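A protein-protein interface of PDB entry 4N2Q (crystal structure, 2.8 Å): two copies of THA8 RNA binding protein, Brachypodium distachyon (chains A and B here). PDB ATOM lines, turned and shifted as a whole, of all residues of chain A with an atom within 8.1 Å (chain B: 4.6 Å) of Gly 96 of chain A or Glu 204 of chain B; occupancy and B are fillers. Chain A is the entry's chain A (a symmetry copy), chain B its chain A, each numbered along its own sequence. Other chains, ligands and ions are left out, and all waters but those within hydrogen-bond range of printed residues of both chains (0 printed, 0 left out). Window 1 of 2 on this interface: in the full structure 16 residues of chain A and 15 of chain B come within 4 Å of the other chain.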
ATOM      1  N   ARG A  64       4.872  35.519 -11.905  1.00  0.00           N
ATOM      2  CA  ARG A  64       6.219  35.280 -11.370  1.00  0.00           C
ATOM      3  C   ARG A  64       6.287  35.389  -9.845  1.00  0.00           C
ATOM      4  O   ARG A  64       7.237  34.892  -9.236  1.00  0.00           O
ATOM      5  CB  ARG A  64       7.220  36.264 -11.980  1.00  0.00           C
ATOM      6  CG  ARG A  64       7.191  36.356 -13.495  1.00  0.00           C
ATOM      7  CD  ARG A  64       7.907  35.191 -14.171  1.00  0.00           C
ATOM      8  NE  ARG A  64       8.007  35.459 -15.609  1.00  0.00           N
ATOM      9  CZ  ARG A  64       8.475  34.621 -16.528  1.00  0.00           C
ATOM     10  NH1 ARG A  64       8.921  33.413 -16.197  1.00  0.00           N
ATOM     11  NH2 ARG A  64       8.493  34.996 -17.797  1.00  0.00           N
ATOM     12  N   MET A  89      13.137  18.334  -9.360  1.00  0.00           N
ATOM     13  CA  MET A  89      13.981  19.281  -8.647  1.00  0.00           C
ATOM     14  C   MET A  89      15.316  19.433  -9.364  1.00  0.00           C
ATOM     15  O   MET A  89      15.741  20.548  -9.671  1.00  0.00           O
ATOM     16  CB  MET A  89      14.225  18.757  -7.237  1.00  0.00           C
ATOM     17  CG  MET A  89      14.307  19.811  -6.165  1.00  0.00           C
ATOM     18  SD  MET A  89      14.319  19.046  -4.543  1.00  0.00           S
ATOM     19  CE  MET A  89      12.753  18.202  -4.481  1.00  0.00           C
ATOM     20  N   ALA A  90      15.963  18.306  -9.652  1.00  0.00           N
ATOM     21  CA  ALA A  90      17.260  18.322 -10.321  1.00  0.00           C
ATOM     22  C   ALA A  90      17.193  18.934 -11.705  1.00  0.00           C
ATOM     23  O   ALA A  90      18.131  19.597 -12.151  1.00  0.00           O
ATOM     24  CB  ALA A  90      17.810  16.926 -10.404  1.00  0.00           C
ATOM     25  N   GLU A  91      16.079  18.732 -12.394  1.00  0.00           N
ATOM     26  CA  GLU A  91      15.927  19.291 -13.738  1.00  0.00           C
ATOM     27  C   GLU A  91      15.794  20.795 -13.680  1.00  0.00           C
ATOM     28  O   GLU A  91      16.355  21.514 -14.516  1.00  0.00           O
ATOM     29  CB  GLU A  91      14.682  18.710 -14.404  1.00  0.00           C
ATOM     30  CG  GLU A  91      14.412  19.219 -15.817  1.00  0.00           C
ATOM     31  CD  GLU A  91      15.582  19.036 -16.771  1.00  0.00           C
ATOM     32  OE1 GLU A  91      16.524  18.276 -16.462  1.00  0.00           O
ATOM     33  OE2 GLU A  91      15.575  19.672 -17.842  1.00  0.00           O
ATOM     34  N   LEU A  92      15.041  21.276 -12.694  1.00  0.00           N
ATOM     35  CA  LEU A  92      14.870  22.721 -12.507  1.00  0.00           C
ATOM     36  C   LEU A  92      16.215  23.373 -12.195  1.00  0.00           C
ATOM     37  O   LEU A  92      16.541  24.428 -12.738  1.00  0.00           O
ATOM     38  CB  LEU A  92      13.873  23.007 -11.389  1.00  0.00           C
ATOM     39  CG  LEU A  92      12.390  22.642 -11.617  1.00  0.00           C
ATOM     40  CD1 LEU A  92      11.617  22.610 -10.298  1.00  0.00           C
ATOM     41  CD2 LEU A  92      11.748  23.640 -12.556  1.00  0.00           C
ATOM     42  N   GLN A  93      17.005  22.724 -11.342  1.00  0.00           N
ATOM     43  CA  GLN A  93      18.334  23.220 -11.008  1.00  0.00           C
ATOM     44  C   GLN A  93      19.147  23.276 -12.263  1.00  0.00           C
ATOM     45  O   GLN A  93      19.755  24.283 -12.557  1.00  0.00           O
ATOM     46  CB  GLN A  93      19.051  22.319  -9.989  1.00  0.00           C
ATOM     47  CG  GLN A  93      18.352  22.229  -8.650  1.00  0.00           C
ATOM     48  CD  GLN A  93      19.111  21.359  -7.678  1.00  0.00           C
ATOM     49  OE1 GLN A  93      19.766  20.425  -8.086  1.00  0.00           O
ATOM     50  NE2 GLN A  93      19.018  21.667  -6.379  1.00  0.00           N
ATOM     51  N   ARG A  94      19.157  22.177 -13.005  1.00  0.00           N
ATOM     52  CA  ARG A  94      19.942  22.089 -14.241  1.00  0.00           C
ATOM     53  C   ARG A  94      19.599  23.193 -15.224  1.00  0.00           C
ATOM     54  O   ARG A  94      20.483  23.768 -15.824  1.00  0.00           O
ATOM     55  CB  ARG A  94      19.726  20.745 -14.893  1.00  0.00           C
ATOM     56  CG  ARG A  94      20.739  20.397 -15.963  1.00  0.00           C
ATOM     57  CD  ARG A  94      20.313  19.123 -16.725  1.00  0.00           C
ATOM     58  NE  ARG A  94      19.097  19.378 -17.508  1.00  0.00           N
ATOM     59  CZ  ARG A  94      19.053  20.163 -18.587  1.00  0.00           C
ATOM     60  NH1 ARG A  94      20.162  20.733 -19.061  1.00  0.00           N
ATOM     61  NH2 ARG A  94      17.891  20.386 -19.197  1.00  0.00           N
ATOM     62  N   GLN A  95      18.310  23.497 -15.360  1.00  0.00           N
ATOM     63  CA  GLN A  95      17.855  24.549 -16.264  1.00  0.00           C
ATOM     64  C   GLN A  95      18.165  25.939 -15.768  1.00  0.00           C
ATOM     65  O   GLN A  95      18.230  26.870 -16.557  1.00  0.00           O
ATOM     66  CB  GLN A  95      16.351  24.438 -16.495  1.00  0.00           C
ATOM     67  CG  GLN A  95      15.983  23.358 -17.490  1.00  0.00           C
ATOM     68  CD  GLN A  95      14.499  23.222 -17.623  1.00  0.00           C
ATOM     69  OE1 GLN A  95      13.748  24.233 -17.603  1.00  0.00           O
ATOM     70  NE2 GLN A  95      14.042  21.968 -17.721  1.00  0.00           N
ATOM     71  N   GLY A  96      18.323  26.090 -14.459  1.00  0.00           N
ATOM     72  CA  GLY A  96      18.655  27.392 -13.878  1.00  0.00           C
ATOM     73  C   GLY A  96      17.521  27.999 -13.079  1.00  0.00           C
ATOM     74  O   GLY A  96      17.676  29.082 -12.510  1.00  0.00           O
ATOM     75  N   HIS A  97      16.379  27.315 -13.020  1.00  0.00           N
ATOM     76  CA  HIS A  97      15.244  27.814 -12.254  1.00  0.00           C
ATOM     77  C   HIS A  97      15.414  27.486 -10.777  1.00  0.00           C
ATOM     78  O   HIS A  97      14.683  26.667 -10.202  1.00  0.00           O
ATOM     79  CB  HIS A  97      13.939  27.229 -12.788  1.00  0.00           C
ATOM     80  CG  HIS A  97      13.602  27.669 -14.183  1.00  0.00           C
ATOM     81  ND1 HIS A  97      13.109  28.924 -14.461  1.00  0.00           N
ATOM     82  CD2 HIS A  97      13.659  27.015 -15.373  1.00  0.00           C
ATOM     83  CE1 HIS A  97      12.886  29.031 -15.761  1.00  0.00           C
ATOM     84  NE2 HIS A  97      13.216  27.889 -16.337  1.00  0.00           N
ATOM     85  N   TRP A  98      16.382  28.147 -10.159  1.00  0.00           N
ATOM     86  CA  TRP A  98      16.754  27.840  -8.768  1.00  0.00           C
ATOM     87  C   TRP A  98      15.601  28.105  -7.790  1.00  0.00           C
ATOM     88  O   TRP A  98      15.290  27.270  -6.938  1.00  0.00           O
ATOM     89  CB  TRP A  98      17.981  28.665  -8.387  1.00  0.00           C
ATOM     90  CG  TRP A  98      18.793  28.083  -7.280  1.00  0.00           C
ATOM     91  CD1 TRP A  98      19.512  26.926  -7.326  1.00  0.00           C
ATOM     92  CD2 TRP A  98      19.016  28.640  -5.974  1.00  0.00           C
ATOM     93  NE1 TRP A  98      20.142  26.713  -6.130  1.00  0.00           N
ATOM     94  CE2 TRP A  98      19.861  27.748  -5.280  1.00  0.00           C
ATOM     95  CE3 TRP A  98      18.563  29.793  -5.311  1.00  0.00           C
ATOM     96  CZ2 TRP A  98      20.261  27.970  -3.950  1.00  0.00           C
ATOM     97  CZ3 TRP A  98      18.959  30.006  -3.979  1.00  0.00           C
ATOM     98  CH2 TRP A  98      19.791  29.101  -3.323  1.00  0.00           C
ATOM     99  N   SER A  99      14.964  29.266  -7.922  1.00  0.00           N
ATOM    100  CA  SER A  99      13.826  29.611  -7.066  1.00  0.00           C
ATOM    101  C   SER A  99      12.729  28.569  -7.156  1.00  0.00           C
ATOM    102  O   SER A  99      12.031  28.314  -6.188  1.00  0.00           O
ATOM    103  CB  SER A  99      13.240  30.997  -7.411  1.00  0.00           C
ATOM    104  OG  SER A  99      12.460  30.976  -8.600  1.00  0.00           O
ATOM    105  N   LEU A 100      12.565  27.984  -8.331  1.00  0.00           N
ATOM    106  CA  LEU A 100      11.560  26.936  -8.521  1.00  0.00           C
ATOM    107  C   LEU A 100      12.030  25.617  -7.892  1.00  0.00           C
ATOM    108  O   LEU A 100      11.237  24.863  -7.300  1.00  0.00           O
ATOM    109  CB  LEU A 100      11.291  26.745 -10.008  1.00  0.00           C
ATOM    110  CG  LEU A 100      10.633  27.931 -10.751  1.00  0.00           C
ATOM    111  CD1 LEU A 100      10.209  27.531 -12.157  1.00  0.00           C
ATOM    112  CD2 LEU A 100       9.445  28.516  -9.997  1.00  0.00           C
ATOM    113  N   ALA A 101      13.324  25.343  -8.015  1.00  0.00           N
ATOM    114  CA  ALA A 101      13.899  24.185  -7.370  1.00  0.00           C
ATOM    115  C   ALA A 101      13.653  24.292  -5.865  1.00  0.00           C
ATOM    116  O   ALA A 101      13.268  23.303  -5.212  1.00  0.00           O
ATOM    117  CB  ALA A 101      15.391  24.107  -7.660  1.00  0.00           C
ATOM    118  N   LEU A 102      13.859  25.490  -5.310  1.00  0.00           N
ATOM    119  CA  LEU A 102      13.598  25.709  -3.872  1.00  0.00           C
ATOM    120  C   LEU A 102      12.127  25.491  -3.531  1.00  0.00           C
ATOM    121  O   LEU A 102      11.790  24.959  -2.468  1.00  0.00           O
ATOM    122  CB  LEU A 102      14.001  27.116  -3.432  1.00  0.00           C
ATOM    123  CG  LEU A 102      15.481  27.453  -3.395  1.00  0.00           C
ATOM    124  CD1 LEU A 102      15.723  28.901  -2.980  1.00  0.00           C
ATOM    125  CD2 LEU A 102      16.184  26.514  -2.443  1.00  0.00           C
ATOM    126  N   SER A 127      24.147  24.493  -7.683  1.00  0.00           N
ATOM    127  CA  SER A 127      23.338  25.124  -8.704  1.00  0.00           C
ATOM    128  C   SER A 127      22.975  26.566  -8.388  1.00  0.00           C
ATOM    129  O   SER A 127      22.417  27.246  -9.231  1.00  0.00           O
ATOM    130  CB  SER A 127      22.069  24.304  -8.926  1.00  0.00           C
ATOM    131  OG  SER A 127      21.352  24.090  -7.719  1.00  0.00           O
ATOM    132  N   SER A 128      23.272  27.034  -7.180  1.00  0.00           N
ATOM    133  CA  SER A 128      22.966  28.440  -6.785  1.00  0.00           C
ATOM    134  C   SER A 128      23.759  29.458  -7.607  1.00  0.00           C
ATOM    135  O   SER A 128      24.915  29.199  -7.929  1.00  0.00           O
ATOM    136  CB  SER A 128      23.293  28.662  -5.304  1.00  0.00           C
ATOM    137  OG  SER A 128      24.705  28.627  -5.107  1.00  0.00           O
ATOM    138  N   PRO A 129      23.146  30.606  -7.952  1.00  0.00           N
ATOM    139  CA  PRO A 129      23.812  31.657  -8.762  1.00  0.00           C
ATOM    140  C   PRO A 129      25.002  32.321  -8.043  1.00  0.00           C
ATOM    141  O   PRO A 129      24.891  32.743  -6.889  1.00  0.00           O
ATOM    142  CB  PRO A 129      22.704  32.696  -9.017  1.00  0.00           C
ATOM    143  CG  PRO A 129      21.423  32.112  -8.523  1.00  0.00           C
ATOM    144  CD  PRO A 129      21.728  30.897  -7.683  1.00  0.00           C
ATOM    145  N   ASP A 132      25.614  36.617  -5.960  1.00  0.00           N
ATOM    146  CA  ASP A 132      24.192  36.849  -5.744  1.00  0.00           C
ATOM    147  C   ASP A 132      23.903  36.916  -4.240  1.00  0.00           C
ATOM    148  O   ASP A 132      23.607  35.890  -3.613  1.00  0.00           O
ATOM    149  CB  ASP A 132      23.394  35.684  -6.364  1.00  0.00           C
ATOM    150  CG  ASP A 132      22.163  36.129  -7.070  1.00  0.00           C
ATOM    151  OD1 ASP A 132      22.246  36.285  -8.332  1.00  0.00           O
ATOM    152  OD2 ASP A 132      21.136  36.325  -6.364  1.00  0.00           O
ATOM    153  N   ASP B 203      13.111  35.334 -16.931  1.00  0.00           N
ATOM    154  CA  ASP B 203      13.294  34.437 -15.797  1.00  0.00           C
ATOM    155  C   ASP B 203      14.754  34.012 -15.619  1.00  0.00           C
ATOM    156  O   ASP B 203      15.644  34.420 -16.363  1.00  0.00           O
ATOM    157  CB  ASP B 203      12.399  33.201 -15.950  1.00  0.00           C
ATOM    158  CG  ASP B 203      12.620  32.460 -17.261  1.00  0.00           C
ATOM    159  OD1 ASP B 203      13.489  32.864 -18.075  1.00  0.00           O
ATOM    160  OD2 ASP B 203      11.887  31.475 -17.500  1.00  0.00           O
ATOM    161  N   GLU B 204      14.977  33.157 -14.634  1.00  0.00           N
ATOM    162  CA  GLU B 204      16.310  32.674 -14.328  1.00  0.00           C
ATOM    163  C   GLU B 204      16.970  32.011 -15.545  1.00  0.00           C
ATOM    164  O   GLU B 204      18.145  32.214 -15.812  1.00  0.00           O
ATOM    165  CB  GLU B 204      16.239  31.699 -13.151  1.00  0.00           C
ATOM    166  CG  GLU B 204      15.952  32.387 -11.829  1.00  0.00           C
ATOM    167  CD  GLU B 204      15.308  31.466 -10.806  1.00  0.00           C
ATOM    168  OE1 GLU B 204      14.170  31.027 -11.061  1.00  0.00           O
ATOM    169  OE2 GLU B 204      15.925  31.187  -9.739  1.00  0.00           O
ATOM    170  N   TYR B 205      16.205  31.227 -16.279  1.00  0.00           N
ATOM    171  CA  TYR B 205      16.700  30.513 -17.452  1.00  0.00           C
ATOM    172  C   TYR B 205      17.339  31.508 -18.408  1.00  0.00           C
ATOM    173  O   TYR B 205      18.454  31.306 -18.854  1.00  0.00           O
ATOM    174  CB  TYR B 205      15.508  29.797 -18.111  1.00  0.00           C
ATOM    175  CG  TYR B 205      15.820  28.817 -19.234  1.00  0.00           C
ATOM    176  CD1 TYR B 205      15.530  27.465 -19.093  1.00  0.00           C
ATOM    177  CD2 TYR B 205      16.363  29.236 -20.437  1.00  0.00           C
ATOM    178  CE1 TYR B 205      15.817  26.545 -20.094  1.00  0.00           C
ATOM    179  CE2 TYR B 205      16.631  28.332 -21.462  1.00  0.00           C
ATOM    180  CZ  TYR B 205      16.356  26.980 -21.279  1.00  0.00           C
ATOM    181  OH  TYR B 205      16.598  26.055 -22.281  1.00  0.00           O
ATOM    182  N   MET B 206      16.629  32.599 -18.702  1.00  0.00           N
ATOM    183  CA  MET B 206      17.152  33.673 -19.572  1.00  0.00           C
ATOM    184  C   MET B 206      18.470  34.274 -19.055  1.00  0.00           C
ATOM    185  O   MET B 206      19.442  34.412 -19.810  1.00  0.00           O
ATOM    186  CB  MET B 206      16.097  34.773 -19.752  1.00  0.00           C
ATOM    187  CG  MET B 206      16.597  36.061 -20.401  1.00  0.00           C
ATOM    188  SD  MET B 206      17.335  35.910 -22.058  1.00  0.00           S
ATOM    189  CE  MET B 206      16.013  36.655 -22.981  1.00  0.00           C
ATOM    190  N   TYR B 207      18.497  34.617 -17.771  1.00  0.00           N
ATOM    191  CA  TYR B 207      19.697  35.170 -17.142  1.00  0.00           C
ATOM    192  C   TYR B 207      20.887  34.243 -17.257  1.00  0.00           C
ATOM    193  O   TYR B 207      21.941  34.640 -17.760  1.00  0.00           O
ATOM    194  CB  TYR B 207      19.443  35.512 -15.667  1.00  0.00           C
ATOM    195  CG  TYR B 207      18.482  36.678 -15.466  1.00  0.00           C
ATOM    196  CD1 TYR B 207      18.767  37.941 -15.992  1.00  0.00           C
ATOM    197  CD2 TYR B 207      17.284  36.513 -14.770  1.00  0.00           C
ATOM    198  CE1 TYR B 207      17.901  39.024 -15.811  1.00  0.00           C
ATOM    199  CE2 TYR B 207      16.415  37.589 -14.584  1.00  0.00           C
ATOM    200  CZ  TYR B 207      16.737  38.840 -15.106  1.00  0.00           C
ATOM    201  OH  TYR B 207      15.884  39.901 -14.965  1.00  0.00           O
ATOM    202  N   ARG B 208      20.702  33.002 -16.829  1.00  0.00           N
ATOM    203  CA  ARG B 208      21.774  31.981 -16.901  1.00  0.00           C
ATOM    204  C   ARG B 208      22.324  31.812 -18.297  1.00  0.00           C
ATOM    205  O   ARG B 208      23.528  31.664 -18.504  1.00  0.00           O
ATOM    206  CB  ARG B 208      21.291  30.622 -16.369  1.00  0.00           C
ATOM    207  CG  ARG B 208      20.719  30.707 -14.946  1.00  0.00           C
ATOM    208  CD  ARG B 208      21.664  31.372 -13.942  1.00  0.00           C
ATOM    209  NE  ARG B 208      22.368  30.379 -13.145  1.00  0.00           N
ATOM    210  CZ  ARG B 208      21.845  29.773 -12.082  1.00  0.00           C
ATOM    211  NH1 ARG B 208      20.607  30.071 -11.680  1.00  0.00           N
ATOM    212  NH2 ARG B 208      22.566  28.875 -11.417  1.00  0.00           N
ATOM    213  N   LEU B 230      20.290  39.491 -12.481  1.00  0.00           N
ATOM    214  CA  LEU B 230      19.812  38.267 -11.890  1.00  0.00           C
ATOM    215  C   LEU B 230      19.716  38.400 -10.375  1.00  0.00           C
ATOM    216  O   LEU B 230      18.749  37.941  -9.756  1.00  0.00           O
ATOM    217  CB  LEU B 230      20.736  37.096 -12.275  1.00  0.00           C
ATOM    218  CG  LEU B 230      20.474  35.756 -11.571  1.00  0.00           C
ATOM    219  CD1 LEU B 230      19.099  35.195 -11.876  1.00  0.00           C
ATOM    220  CD2 LEU B 230      21.525  34.758 -12.004  1.00  0.00           C
ATOM    221  N   TRP B 233      16.758  40.252  -9.452  1.00  0.00           N
ATOM    222  CA  TRP B 233      15.593  39.394  -9.677  1.00  0.00           C
ATOM    223  C   TRP B 233      15.396  38.471  -8.500  1.00  0.00           C
ATOM    224  O   TRP B 233      14.306  38.409  -7.911  1.00  0.00           O
ATOM    225  CB  TRP B 233      15.785  38.580 -10.958  1.00  0.00           C
ATOM    226  CG  TRP B 233      14.563  37.847 -11.405  1.00  0.00           C
ATOM    227  CD1 TRP B 233      13.645  38.260 -12.339  1.00  0.00           C
ATOM    228  CD2 TRP B 233      14.104  36.570 -10.933  1.00  0.00           C
ATOM    229  NE1 TRP B 233      12.646  37.324 -12.461  1.00  0.00           N
ATOM    230  CE2 TRP B 233      12.912  36.272 -11.621  1.00  0.00           C
ATOM    231  CE3 TRP B 233      14.586  35.647  -9.998  1.00  0.00           C
ATOM    232  CZ2 TRP B 233      12.203  35.087 -11.405  1.00  0.00           C
ATOM    233  CZ3 TRP B 233      13.875  34.468  -9.795  1.00  0.00           C
ATOM    234  CH2 TRP B 233      12.703  34.204 -10.489  1.00  0.00           C
ATOM    235  N   GLU B 234      16.478  37.784  -8.140  1.00  0.00           N
ATOM    236  CA  GLU B 234      16.474  36.868  -7.004  1.00  0.00           C
ATOM    237  C   GLU B 234      16.060  37.572  -5.720  1.00  0.00           C
ATOM    238  O   GLU B 234      15.321  37.033  -4.907  1.00  0.00           O
ATOM    239  CB  GLU B 234      17.860  36.225  -6.831  1.00  0.00           C
ATOM    240  CG  GLU B 234      18.272  35.274  -7.948  1.00  0.00           C
ATOM    241  CD  GLU B 234      17.416  34.007  -8.032  1.00  0.00           C
ATOM    242  OE1 GLU B 234      16.457  33.862  -7.244  1.00  0.00           O
ATOM    243  OE2 GLU B 234      17.714  33.138  -8.879  1.00  0.00           O
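No position is printed for both chains.
Gly 96 of chain A touches just these residues of chain B: Glu 204 and Arg 208. Glu 204 of chain B touches just these residues of chain A: Gly 96 (3.1 Å), His 97 (3.6 Å), Trp 98 (3.1 Å) and Ser 99 (2.8 Å). Of the printed residues of chain A, Trp 233 of chain B touches Ser 99. Of the printed residues of chain A, Arg 208 of chain B touches Gly 96, Ser 127 and Pro 129. Printed residues of chain B within 4 Å of Trp 98 of chain A: Glu 204. Leu 92 of chain A touches none of the printed residues of chain B. The nearest residue of chain A that does not touch Glu 204 of chain B is Leu 100 of chain A (4.4 Å).
The side-chain carboxylate (OE2) of Glu 204 of chain B is in hydrogen-bond range of the backbone NH (N) of Trp 98 of chain A. NH1 of Arg 64 of chain A is in salt-bridge range of OD2 of Asp 203 of chain B, at 3.8 Å. The guanidinium group (NH1) of Arg 208 of chain B is in hydrogen-bond range of the backbone carbonyl oxygen (O) of Gly 96 of chain A (3.2 Å). The backbone NH (N) of Ser 99 of chain A sits at hydrogen-bond distance from the side-chain carboxylate (OE2) of Glu 204 of chain B, at 2.8 Å. NH2 of Arg 208 of chain B is in hydrogen-bond range of O of Ser 127 of chain A, at 2.7 Å.
Among the printed residues, merely in contact across the chains: Gln 95 of chain A with Tyr 205 of chain B (3.8 Å), Gly 96 of chain A with Glu 204 of chain B (3.1 Å), His 97 of chain A with Asp 203 of chain B (3.2 Å), His 97 of chain A with Glu 204 of chain B (3.6 Å), His 97 of chain A with Tyr 205 of chain B (3.5 Å), Ser 99 of chain A with Trp 233 of chain B (3.7 Å), Pro 129 of chain A with Arg 208 of chain B (3.8 Å), Pro 129 of chain A with Leu 230 of chain B (3.8 Å), Pro 129 of chain A with Glu 234 of chain B (3.9 Å), Asp 132 of chain A with Leu 230 of chain B (3.7 Å) and Asp 132 of chain A with Glu 234 of chain B (3.3 Å).
Hydrophobic or aromatic side chains of chain B within 4 Å of the printed part of chain A: Tyr 205, Leu 230 and Trp 233. Of the 19 printed residues of chain A, 9 touch a printed residue of chain B. Printed residues of chain A that touch a printed residue of chain B: Arg 64, Gln 95, Gly 96, His 97, Trp 98, Ser 99, Ser 127, Pro 129 and Asp 132. Hydrophobic or aromatic side chains of chain A within 4 Å of the printed part of chain B: His 97, Trp 98 and Pro 129. Among the printed residues, 16 pairs touch across the chains.
The side-chain carboxylate (OD1) of Asp 203 of chain B sits at hydrogen-bond distance from the backbone NH (N) of Met 206 of chain B. The indole nitrogen (NE1) of Trp 98 of chain A lies within hydrogen-bond range of the side-chain hydroxyl (OG) of Ser 127 of chain A, 3.3 Å away. The side-chain amide nitrogen (NE2) of Gln 95 of chain A is in hydrogen-bond range of the side-chain carboxylate (OE2) of Glu 91 of chain A. O of Leu 92 of chain A is in hydrogen-bond range of N of His 97 of chain A (2.9 Å).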
